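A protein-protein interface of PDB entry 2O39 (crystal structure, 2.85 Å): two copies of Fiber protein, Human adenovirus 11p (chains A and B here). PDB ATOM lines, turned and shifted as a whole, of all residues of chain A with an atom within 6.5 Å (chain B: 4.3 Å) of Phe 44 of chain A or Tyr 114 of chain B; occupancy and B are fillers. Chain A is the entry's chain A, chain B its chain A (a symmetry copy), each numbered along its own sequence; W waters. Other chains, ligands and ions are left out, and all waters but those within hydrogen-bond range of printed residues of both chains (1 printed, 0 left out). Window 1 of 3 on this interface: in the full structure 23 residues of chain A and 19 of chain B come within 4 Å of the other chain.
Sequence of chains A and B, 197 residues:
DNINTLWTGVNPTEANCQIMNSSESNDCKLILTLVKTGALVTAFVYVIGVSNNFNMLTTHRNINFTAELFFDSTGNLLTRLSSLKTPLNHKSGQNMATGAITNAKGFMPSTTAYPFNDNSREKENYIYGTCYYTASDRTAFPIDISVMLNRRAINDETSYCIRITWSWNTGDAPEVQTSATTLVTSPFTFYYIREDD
The backbone carbonyl oxygen of Thr 33 of chain A is in hydrogen-bond range of the backbone NH of Phe 44 of chain A, 2.8 Å away.
OG of Ser 110 of chain B is in hydrogen-bond range of N of Thr 112 of chain B, 2.9 Å away.
N of Ala 113 of chain B is in hydrogen-bond range of OG of Ser 110 of chain B, at 2.9 Å.
The backbone carbonyl oxygen (O) of Ile 193 of chain B lies within hydrogen-bond range of the backbone NH (N) of Ser 110 of chain B, at 3.0 Å.
O of Tyr 114 of chain B sits at hydrogen-bond distance from ND2 of Asn 150 of chain B (2.6 Å).
N of Ile 193 of chain B sits at hydrogen-bond distance from OH of Tyr 114 of chain B.
Thr 112 of chain B touches Val 10 of chain A (CG2 to CG1, 3.6 Å).
Val 10 of chain A touches Ala 113 of chain B.
Val 10 of chain A touches Ile 193 of chain B.
CB of Phe 44 of chain A touches CD1 of Leu 40 of chain B (3.6 Å).
OH of Tyr 114 of chain B touches CZ of Phe 44 of chain A, 3.996 Å away.
Phe 44 of chain A touches Tyr 191 of chain B.
Ile 193 of chain B touches Phe 44 of chain A (CD1 to CE2, 3.6 Å).
OG1 of Thr 189 of chain A touches CD2 of Tyr 191 of chain B, at 3.3 Å.
Of the printed residues of chain B, Phe 44 of chain A touches Leu 40 (3.6 Å), Tyr 114 (3.996 Å), Tyr 191 (3.7 Å) and Ile 193 (3.6 Å).
Of the printed residues of chain A, Tyr 114 of chain B touches Phe 44 (3.996 Å).
Printed residues of chain A within 4 Å of Thr 112 of chain B: Val 10.
Of the printed residues of chain A, Ile 193 of chain B touches Val 10 and Phe 44.
Of the printed residues of chain A, Leu 40 of chain B touches Phe 44.
Of the printed residues of chain A, Ala 113 of chain B touches Val 10.
Printed residues of chain A within 4 Å of Tyr 191 of chain B: Phe 44 (3.7 Å) and Thr 189 (3.3 Å).
Tyr 192 of chain B touches none of the printed residues of chain A.
Of the 15 printed residues of chain A, 3 touch a printed residue of chain B.
Hydrophobic or aromatic side chains of chain A within 4 Å of the printed part of chain B: Val 10 and Phe 44.
Hydrophobic or aromatic side chains of chain B within 4 Å of the printed part of chain A: Leu 40, Ala 113, Tyr 114, Tyr 191 and Ile 193.
Along chain B the printed residues that touch a printed residue of chain A span positions 40 to 193.
No position is printed for both chains.
Water W1 lies within hydrogen-bond range of OE1 of Glu 124 of chain B, O of Ala 113 of chain B and OH of Tyr 46 of chain A.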
ATOM      1  N   VAL A  10     -10.636  -2.865 -15.213  1.00  0.00           N
ATOM      2  CA  VAL A  10     -12.086  -2.775 -15.313  1.00  0.00           C
ATOM      3  C   VAL A  10     -12.773  -2.799 -13.951  1.00  0.00           C
ATOM      4  O   VAL A  10     -12.330  -3.497 -13.028  1.00  0.00           O
ATOM      5  CB  VAL A  10     -12.643  -3.921 -16.167  1.00  0.00           C
ATOM      6  CG1 VAL A  10     -14.123  -3.720 -16.412  1.00  0.00           C
ATOM      7  CG2 VAL A  10     -11.897  -3.988 -17.471  1.00  0.00           C
ATOM      8  N   ILE A  31     -12.709   5.051 -13.911  1.00  0.00           N
ATOM      9  CA  ILE A  31     -12.117   4.120 -14.862  1.00  0.00           C
ATOM     10  C   ILE A  31     -11.340   4.906 -15.928  1.00  0.00           C
ATOM     11  O   ILE A  31     -11.899   5.783 -16.607  1.00  0.00           O
ATOM     12  CB  ILE A  31     -13.187   3.272 -15.551  1.00  0.00           C
ATOM     13  CG1 ILE A  31     -13.727   2.219 -14.589  1.00  0.00           C
ATOM     14  CG2 ILE A  31     -12.597   2.558 -16.729  1.00  0.00           C
ATOM     15  CD1 ILE A  31     -14.620   2.746 -13.521  1.00  0.00           C
ATOM     16  N   LEU A  32     -10.049   4.602 -16.065  1.00  0.00           N
ATOM     17  CA  LEU A  32      -9.215   5.288 -17.056  1.00  0.00           C
ATOM     18  C   LEU A  32      -8.310   4.356 -17.857  1.00  0.00           C
ATOM     19  O   LEU A  32      -7.585   3.533 -17.299  1.00  0.00           O
ATOM     20  CB  LEU A  32      -8.359   6.359 -16.391  1.00  0.00           C
ATOM     21  CG  LEU A  32      -7.463   7.119 -17.366  1.00  0.00           C
ATOM     22  CD1 LEU A  32      -8.307   7.820 -18.399  1.00  0.00           C
ATOM     23  CD2 LEU A  32      -6.625   8.117 -16.602  1.00  0.00           C
ATOM     24  N   THR A  33      -8.348   4.523 -19.176  1.00  0.00           N
ATOM     25  CA  THR A  33      -7.563   3.707 -20.083  1.00  0.00           C
ATOM     26  C   THR A  33      -6.826   4.561 -21.129  1.00  0.00           C
ATOM     27  O   THR A  33      -7.437   5.256 -21.947  1.00  0.00           O
ATOM     28  CB  THR A  33      -8.480   2.693 -20.791  1.00  0.00           C
ATOM     29  OG1 THR A  33      -9.246   1.999 -19.802  1.00  0.00           O
ATOM     30  CG2 THR A  33      -7.681   1.684 -21.598  1.00  0.00           C
ATOM     31  N   LEU A  34      -5.499   4.511 -21.068  1.00  0.00           N
ATOM     32  CA  LEU A  34      -4.638   5.213 -22.001  1.00  0.00           C
ATOM     33  C   LEU A  34      -4.008   4.117 -22.871  1.00  0.00           C
ATOM     34  O   LEU A  34      -3.374   3.198 -22.361  1.00  0.00           O
ATOM     35  CB  LEU A  34      -3.544   5.961 -21.245  1.00  0.00           C
ATOM     36  CG  LEU A  34      -3.923   6.752 -19.989  1.00  0.00           C
ATOM     37  CD1 LEU A  34      -2.727   7.559 -19.527  1.00  0.00           C
ATOM     38  CD2 LEU A  34      -5.084   7.669 -20.275  1.00  0.00           C
ATOM     39  N   VAL A  35      -4.193   4.200 -24.179  1.00  0.00           N
ATOM     40  CA  VAL A  35      -3.626   3.201 -25.075  1.00  0.00           C
ATOM     41  C   VAL A  35      -2.701   3.852 -26.091  1.00  0.00           C
ATOM     42  O   VAL A  35      -3.042   4.867 -26.697  1.00  0.00           O
ATOM     43  CB  VAL A  35      -4.744   2.438 -25.823  1.00  0.00           C
ATOM     44  CG1 VAL A  35      -4.146   1.452 -26.837  1.00  0.00           C
ATOM     45  CG2 VAL A  35      -5.612   1.701 -24.811  1.00  0.00           C
ATOM     46  N   THR A  42      -4.821   7.283 -26.894  1.00  0.00           N
ATOM     47  CA  THR A  42      -6.270   7.248 -26.900  1.00  0.00           C
ATOM     48  C   THR A  42      -6.652   7.216 -25.427  1.00  0.00           C
ATOM     49  O   THR A  42      -6.294   6.292 -24.707  1.00  0.00           O
ATOM     50  CB  THR A  42      -6.802   5.977 -27.633  1.00  0.00           C
ATOM     51  OG1 THR A  42      -6.366   5.987 -29.001  1.00  0.00           O
ATOM     52  CG2 THR A  42      -8.325   5.935 -27.602  1.00  0.00           C
ATOM     53  N   ALA A  43      -7.342   8.251 -24.972  1.00  0.00           N
ATOM     54  CA  ALA A  43      -7.759   8.324 -23.581  1.00  0.00           C
ATOM     55  C   ALA A  43      -9.225   7.940 -23.529  1.00  0.00           C
ATOM     56  O   ALA A  43     -10.044   8.461 -24.283  1.00  0.00           O
ATOM     57  CB  ALA A  43      -7.560   9.727 -23.052  1.00  0.00           C
ATOM     58  N   PHE A  44      -9.544   7.014 -22.633  1.00  0.00           N
ATOM     59  CA  PHE A  44     -10.902   6.500 -22.466  1.00  0.00           C
ATOM     60  C   PHE A  44     -11.219   6.691 -21.004  1.00  0.00           C
ATOM     61  O   PHE A  44     -10.529   6.137 -20.157  1.00  0.00           O
ATOM     62  CB  PHE A  44     -10.905   5.016 -22.814  1.00  0.00           C
ATOM     63  CG  PHE A  44     -12.238   4.368 -22.714  1.00  0.00           C
ATOM     64  CD1 PHE A  44     -13.182   4.534 -23.725  1.00  0.00           C
ATOM     65  CD2 PHE A  44     -12.530   3.539 -21.635  1.00  0.00           C
ATOM     66  CE1 PHE A  44     -14.403   3.881 -23.674  1.00  0.00           C
ATOM     67  CE2 PHE A  44     -13.737   2.881 -21.559  1.00  0.00           C
ATOM     68  CZ  PHE A  44     -14.684   3.047 -22.588  1.00  0.00           C
ATOM     69  N   VAL A  45     -12.254   7.460 -20.694  1.00  0.00           N
ATOM     70  CA  VAL A  45     -12.553   7.705 -19.291  1.00  0.00           C
ATOM     71  C   VAL A  45     -14.006   7.987 -18.975  1.00  0.00           C
ATOM     72  O   VAL A  45     -14.748   8.519 -19.809  1.00  0.00           O
ATOM     73  CB  VAL A  45     -11.724   8.888 -18.758  1.00  0.00           C
ATOM     74  CG1 VAL A  45     -12.175  10.170 -19.399  1.00  0.00           C
ATOM     75  CG2 VAL A  45     -11.865   8.984 -17.291  1.00  0.00           C
ATOM     76  N   TYR A  46     -14.393   7.602 -17.760  1.00  0.00           N
ATOM     77  CA  TYR A  46     -15.739   7.824 -17.230  1.00  0.00           C
ATOM     78  C   TYR A  46     -15.723   7.545 -15.723  1.00  0.00           C
ATOM     79  O   TYR A  46     -14.693   7.133 -15.176  1.00  0.00           O
ATOM     80  CB  TYR A  46     -16.773   6.941 -17.937  1.00  0.00           C
ATOM     81  CG  TYR A  46     -16.615   5.455 -17.737  1.00  0.00           C
ATOM     82  CD1 TYR A  46     -15.616   4.741 -18.390  1.00  0.00           C
ATOM     83  CD2 TYR A  46     -17.504   4.747 -16.918  1.00  0.00           C
ATOM     84  CE1 TYR A  46     -15.510   3.348 -18.242  1.00  0.00           C
ATOM     85  CE2 TYR A  46     -17.405   3.366 -16.759  1.00  0.00           C
ATOM     86  CZ  TYR A  46     -16.408   2.670 -17.425  1.00  0.00           C
ATOM     87  OH  TYR A  46     -16.320   1.302 -17.288  1.00  0.00           O
ATOM     88  N   PRO A 187     -18.541   6.523 -21.384  1.00  0.00           N
ATOM     89  CA  PRO A 187     -17.137   6.629 -21.765  1.00  0.00           C
ATOM     90  C   PRO A 187     -16.902   7.870 -22.612  1.00  0.00           C
ATOM     91  O   PRO A 187     -17.647   8.114 -23.565  1.00  0.00           O
ATOM     92  CB  PRO A 187     -16.913   5.364 -22.582  1.00  0.00           C
ATOM     93  CG  PRO A 187     -17.875   4.410 -22.028  1.00  0.00           C
ATOM     94  CD  PRO A 187     -19.106   5.248 -21.854  1.00  0.00           C
ATOM     95  N   PHE A 188     -15.896   8.667 -22.255  1.00  0.00           N
ATOM     96  CA  PHE A 188     -15.546   9.843 -23.047  1.00  0.00           C
ATOM     97  C   PHE A 188     -14.141   9.576 -23.559  1.00  0.00           C
ATOM     98  O   PHE A 188     -13.197   9.462 -22.778  1.00  0.00           O
ATOM     99  CB  PHE A 188     -15.539  11.120 -22.222  1.00  0.00           C
ATOM    100  CG  PHE A 188     -15.040  12.315 -22.983  1.00  0.00           C
ATOM    101  CD1 PHE A 188     -15.794  12.867 -24.017  1.00  0.00           C
ATOM    102  CD2 PHE A 188     -13.810  12.895 -22.664  1.00  0.00           C
ATOM    103  CE1 PHE A 188     -15.336  13.979 -24.721  1.00  0.00           C
ATOM    104  CE2 PHE A 188     -13.338  14.010 -23.363  1.00  0.00           C
ATOM    105  CZ  PHE A 188     -14.108  14.553 -24.397  1.00  0.00           C
ATOM    106  N   THR A 189     -14.012   9.472 -24.878  1.00  0.00           N
ATOM    107  CA  THR A 189     -12.734   9.174 -25.508  1.00  0.00           C
ATOM    108  C   THR A 189     -12.150  10.388 -26.195  1.00  0.00           C
ATOM    109  O   THR A 189     -12.791  10.984 -27.043  1.00  0.00           O
ATOM    110  CB  THR A 189     -12.893   8.039 -26.550  1.00  0.00           C
ATOM    111  OG1 THR A 189     -13.472   6.892 -25.917  1.00  0.00           O
ATOM    112  CG2 THR A 189     -11.550   7.646 -27.133  1.00  0.00           C
ATOM    113  N   PHE A 190     -10.932  10.763 -25.818  1.00  0.00           N
ATOM    114  CA  PHE A 190     -10.285  11.896 -26.439  1.00  0.00           C
ATOM    115  C   PHE A 190      -8.878  11.504 -26.827  1.00  0.00           C
ATOM    116  O   PHE A 190      -8.419  10.428 -26.446  1.00  0.00           O
ATOM    117  CB  PHE A 190     -10.302  13.114 -25.511  1.00  0.00           C
ATOM    118  CG  PHE A 190      -9.572  12.926 -24.216  1.00  0.00           C
ATOM    119  CD1 PHE A 190      -8.239  13.287 -24.102  1.00  0.00           C
ATOM    120  CD2 PHE A 190     -10.243  12.456 -23.085  1.00  0.00           C
ATOM    121  CE1 PHE A 190      -7.578  13.195 -22.881  1.00  0.00           C
ATOM    122  CE2 PHE A 190      -9.592  12.358 -21.857  1.00  0.00           C
ATOM    123  CZ  PHE A 190      -8.253  12.731 -21.754  1.00  0.00           C
ATOM    124  N   LEU B  40      -9.051  -1.755 -25.460  1.00  0.00           N
ATOM    125  CA  LEU B  40     -10.304  -1.303 -26.050  1.00  0.00           C
ATOM    126  C   LEU B  40     -10.527  -1.815 -27.478  1.00  0.00           C
ATOM    127  O   LEU B  40      -9.633  -2.378 -28.122  1.00  0.00           O
ATOM    128  CB  LEU B  40     -10.338   0.214 -26.113  1.00  0.00           C
ATOM    129  CG  LEU B  40     -10.043   1.022 -24.868  1.00  0.00           C
ATOM    130  CD1 LEU B  40     -10.041   2.486 -25.259  1.00  0.00           C
ATOM    131  CD2 LEU B  40     -11.069   0.738 -23.801  1.00  0.00           C
ATOM    132  N   PRO B 109     -17.761  -7.078 -26.613  1.00  0.00           N
ATOM    133  CA  PRO B 109     -17.830  -6.107 -25.526  1.00  0.00           C
ATOM    134  C   PRO B 109     -17.776  -6.832 -24.188  1.00  0.00           C
ATOM    135  O   PRO B 109     -18.707  -7.548 -23.822  1.00  0.00           O
ATOM    136  CB  PRO B 109     -19.169  -5.428 -25.766  1.00  0.00           C
ATOM    137  CG  PRO B 109     -19.987  -6.521 -26.333  1.00  0.00           C
ATOM    138  CD  PRO B 109     -19.049  -7.168 -27.316  1.00  0.00           C
ATOM    139  N   SER B 110     -16.669  -6.647 -23.472  1.00  0.00           N
ATOM    140  CA  SER B 110     -16.456  -7.262 -22.159  1.00  0.00           C
ATOM    141  C   SER B 110     -17.687  -7.365 -21.273  1.00  0.00           C
ATOM    142  O   SER B 110     -18.378  -6.371 -21.037  1.00  0.00           O
ATOM    143  CB  SER B 110     -15.405  -6.495 -21.374  1.00  0.00           C
ATOM    144  OG  SER B 110     -15.567  -6.744 -19.984  1.00  0.00           O
ATOM    145  N   THR B 111     -17.943  -8.568 -20.766  1.00  0.00           N
ATOM    146  CA  THR B 111     -19.077  -8.778 -19.870  1.00  0.00           C
ATOM    147  C   THR B 111     -18.745  -8.212 -18.487  1.00  0.00           C
ATOM    148  O   THR B 111     -19.644  -7.918 -17.707  1.00  0.00           O
ATOM    149  CB  THR B 111     -19.419 -10.263 -19.740  1.00  0.00           C
ATOM    150  OG1 THR B 111     -18.221 -11.003 -19.493  1.00  0.00           O
ATOM    151  CG2 THR B 111     -20.066 -10.777 -21.021  1.00  0.00           C
ATOM    152  N   THR B 112     -17.449  -8.055 -18.203  1.00  0.00           N
ATOM    153  CA  THR B 112     -16.985  -7.502 -16.931  1.00  0.00           C
ATOM    154  C   THR B 112     -17.308  -6.007 -16.877  1.00  0.00           C
ATOM    155  O   THR B 112     -17.775  -5.497 -15.862  1.00  0.00           O
ATOM    156  CB  THR B 112     -15.448  -7.685 -16.749  1.00  0.00           C
ATOM    157  OG1 THR B 112     -15.112  -9.077 -16.787  1.00  0.00           O
ATOM    158  CG2 THR B 112     -14.994  -7.114 -15.414  1.00  0.00           C
ATOM    159  N   ALA B 113     -17.050  -5.308 -17.976  1.00  0.00           N
ATOM    160  CA  ALA B 113     -17.323  -3.882 -18.057  1.00  0.00           C
ATOM    161  C   ALA B 113     -18.790  -3.591 -18.375  1.00  0.00           C
ATOM    162  O   ALA B 113     -19.351  -2.615 -17.896  1.00  0.00           O
ATOM    163  CB  ALA B 113     -16.455  -3.268 -19.095  1.00  0.00           C
ATOM    164  N   TYR B 114     -19.403  -4.432 -19.195  1.00  0.00           N
ATOM    165  CA  TYR B 114     -20.808  -4.265 -19.574  1.00  0.00           C
ATOM    166  C   TYR B 114     -21.435  -5.604 -19.271  1.00  0.00           C
ATOM    167  O   TYR B 114     -21.319  -6.551 -20.045  1.00  0.00           O
ATOM    168  CB  TYR B 114     -20.926  -3.935 -21.064  1.00  0.00           C
ATOM    169  CG  TYR B 114     -19.863  -2.974 -21.504  1.00  0.00           C
ATOM    170  CD1 TYR B 114     -18.730  -3.424 -22.173  1.00  0.00           C
ATOM    171  CD2 TYR B 114     -19.939  -1.630 -21.159  1.00  0.00           C
ATOM    172  CE1 TYR B 114     -17.685  -2.554 -22.480  1.00  0.00           C
ATOM    173  CE2 TYR B 114     -18.914  -0.758 -21.458  1.00  0.00           C
ATOM    174  CZ  TYR B 114     -17.784  -1.226 -22.114  1.00  0.00           C
ATOM    175  OH  TYR B 114     -16.732  -0.376 -22.352  1.00  0.00           O
ATOM    176  N   PRO B 115     -22.102  -5.697 -18.122  1.00  0.00           N
ATOM    177  CA  PRO B 115     -22.744  -6.933 -17.687  1.00  0.00           C
ATOM    178  C   PRO B 115     -24.155  -7.213 -18.173  1.00  0.00           C
ATOM    179  O   PRO B 115     -24.782  -6.411 -18.877  1.00  0.00           O
ATOM    180  CB  PRO B 115     -22.688  -6.804 -16.174  1.00  0.00           C
ATOM    181  CG  PRO B 115     -23.007  -5.340 -15.995  1.00  0.00           C
ATOM    182  CD  PRO B 115     -22.169  -4.668 -17.067  1.00  0.00           C
ATOM    183  N   GLU B 124     -24.201   1.757 -16.924  1.00  0.00           N
ATOM    184  CA  GLU B 124     -22.901   1.503 -17.528  1.00  0.00           C
ATOM    185  C   GLU B 124     -22.921   0.757 -18.858  1.00  0.00           C
ATOM    186  O   GLU B 124     -21.869   0.572 -19.472  1.00  0.00           O
ATOM    187  CB  GLU B 124     -22.037   0.724 -16.549  1.00  0.00           C
ATOM    188  CG  GLU B 124     -21.942   1.362 -15.187  1.00  0.00           C
ATOM    189  CD  GLU B 124     -21.293   0.441 -14.167  1.00  0.00           C
ATOM    190  OE1 GLU B 124     -20.282  -0.209 -14.527  1.00  0.00           O
ATOM    191  OE2 GLU B 124     -21.782   0.376 -13.013  1.00  0.00           O
ATOM    192  N   ASN B 125     -24.106   0.329 -19.297  1.00  0.00           N
ATOM    193  CA  ASN B 125     -24.261  -0.416 -20.555  1.00  0.00           C
ATOM    194  C   ASN B 125     -24.576   0.466 -21.765  1.00  0.00           C
ATOM    195  O   ASN B 125     -24.877  -0.042 -22.841  1.00  0.00           O
ATOM    196  CB  ASN B 125     -25.389  -1.445 -20.429  1.00  0.00           C
ATOM    197  CG  ASN B 125     -25.055  -2.590 -19.487  1.00  0.00           C
ATOM    198  OD1 ASN B 125     -25.384  -2.560 -18.289  1.00  0.00           O
ATOM    199  ND2 ASN B 125     -24.394  -3.614 -20.027  1.00  0.00           N
ATOM    200  N   LEU B 149     -24.589  -2.043 -24.910  1.00  0.00           N
ATOM    201  CA  LEU B 149     -23.649  -3.158 -24.908  1.00  0.00           C
ATOM    202  C   LEU B 149     -24.185  -4.301 -24.055  1.00  0.00           C
ATOM    203  O   LEU B 149     -24.424  -4.149 -22.856  1.00  0.00           O
ATOM    204  CB  LEU B 149     -22.279  -2.698 -24.399  1.00  0.00           C
ATOM    205  CG  LEU B 149     -21.624  -1.623 -25.269  1.00  0.00           C
ATOM    206  CD1 LEU B 149     -20.279  -1.209 -24.672  1.00  0.00           C
ATOM    207  CD2 LEU B 149     -21.452  -2.163 -26.689  1.00  0.00           C
ATOM    208  N   ASN B 150     -24.365  -5.445 -24.704  1.00  0.00           N
ATOM    209  CA  ASN B 150     -24.899  -6.667 -24.102  1.00  0.00           C
ATOM    210  C   ASN B 150     -25.514  -6.593 -22.699  1.00  0.00           C
ATOM    211  O   ASN B 150     -24.947  -7.115 -21.745  1.00  0.00           O
ATOM    212  CB  ASN B 150     -23.836  -7.792 -24.175  1.00  0.00           C
ATOM    213  CG  ASN B 150     -22.553  -7.485 -23.395  1.00  0.00           C
ATOM    214  OD1 ASN B 150     -21.463  -7.827 -23.840  1.00  0.00           O
ATOM    215  ND2 ASN B 150     -22.681  -6.883 -22.233  1.00  0.00           N
ATOM    216  N   TYR B 191     -16.157   3.630 -28.604  1.00  0.00           N
ATOM    217  CA  TYR B 191     -15.218   2.748 -27.913  1.00  0.00           C
ATOM    218  C   TYR B 191     -15.813   1.937 -26.772  1.00  0.00           C
ATOM    219  O   TYR B 191     -16.795   2.351 -26.147  1.00  0.00           O
ATOM    220  CB  TYR B 191     -14.074   3.582 -27.350  1.00  0.00           C
ATOM    221  CG  TYR B 191     -13.280   4.291 -28.407  1.00  0.00           C
ATOM    222  CD1 TYR B 191     -12.181   3.669 -29.002  1.00  0.00           C
ATOM    223  CD2 TYR B 191     -13.675   5.545 -28.878  1.00  0.00           C
ATOM    224  CE1 TYR B 191     -11.499   4.269 -30.039  1.00  0.00           C
ATOM    225  CE2 TYR B 191     -13.004   6.155 -29.916  1.00  0.00           C
ATOM    226  CZ  TYR B 191     -11.917   5.510 -30.494  1.00  0.00           C
ATOM    227  OH  TYR B 191     -11.245   6.105 -31.530  1.00  0.00           O
ATOM    228  N   TYR B 192     -15.206   0.782 -26.499  1.00  0.00           N
ATOM    229  CA  TYR B 192     -15.653  -0.060 -25.404  1.00  0.00           C
ATOM    230  C   TYR B 192     -14.568  -1.028 -24.978  1.00  0.00           C
ATOM    231  O   TYR B 192     -13.725  -1.416 -25.787  1.00  0.00           O
ATOM    232  CB  TYR B 192     -16.949  -0.815 -25.766  1.00  0.00           C
ATOM    233  CG  TYR B 192     -16.867  -1.859 -26.880  1.00  0.00           C
ATOM    234  CD1 TYR B 192     -16.150  -3.046 -26.710  1.00  0.00           C
ATOM    235  CD2 TYR B 192     -17.543  -1.675 -28.090  1.00  0.00           C
ATOM    236  CE1 TYR B 192     -16.111  -4.023 -27.720  1.00  0.00           C
ATOM    237  CE2 TYR B 192     -17.507  -2.640 -29.101  1.00  0.00           C
ATOM    238  CZ  TYR B 192     -16.789  -3.809 -28.910  1.00  0.00           C
ATOM    239  OH  TYR B 192     -16.728  -4.749 -29.914  1.00  0.00           O
ATOM    240  N   ILE B 193     -14.581  -1.383 -23.689  1.00  0.00           N
ATOM    241  CA  ILE B 193     -13.616  -2.324 -23.112  1.00  0.00           C
ATOM    242  C   ILE B 193     -13.928  -3.682 -23.705  1.00  0.00           C
ATOM    243  O   ILE B 193     -15.093  -4.083 -23.731  1.00  0.00           O
ATOM    244  CB  ILE B 193     -13.772  -2.458 -21.588  1.00  0.00           C
ATOM    245  CG1 ILE B 193     -13.698  -1.088 -20.914  1.00  0.00           C
ATOM    246  CG2 ILE B 193     -12.671  -3.368 -21.044  1.00  0.00           C
ATOM    247  CD1 ILE B 193     -12.353  -0.414 -21.033  1.00  0.00           C
HETATM  248  O   HOH W   1     -18.163  -0.671 -16.216  1.00  0.00           O
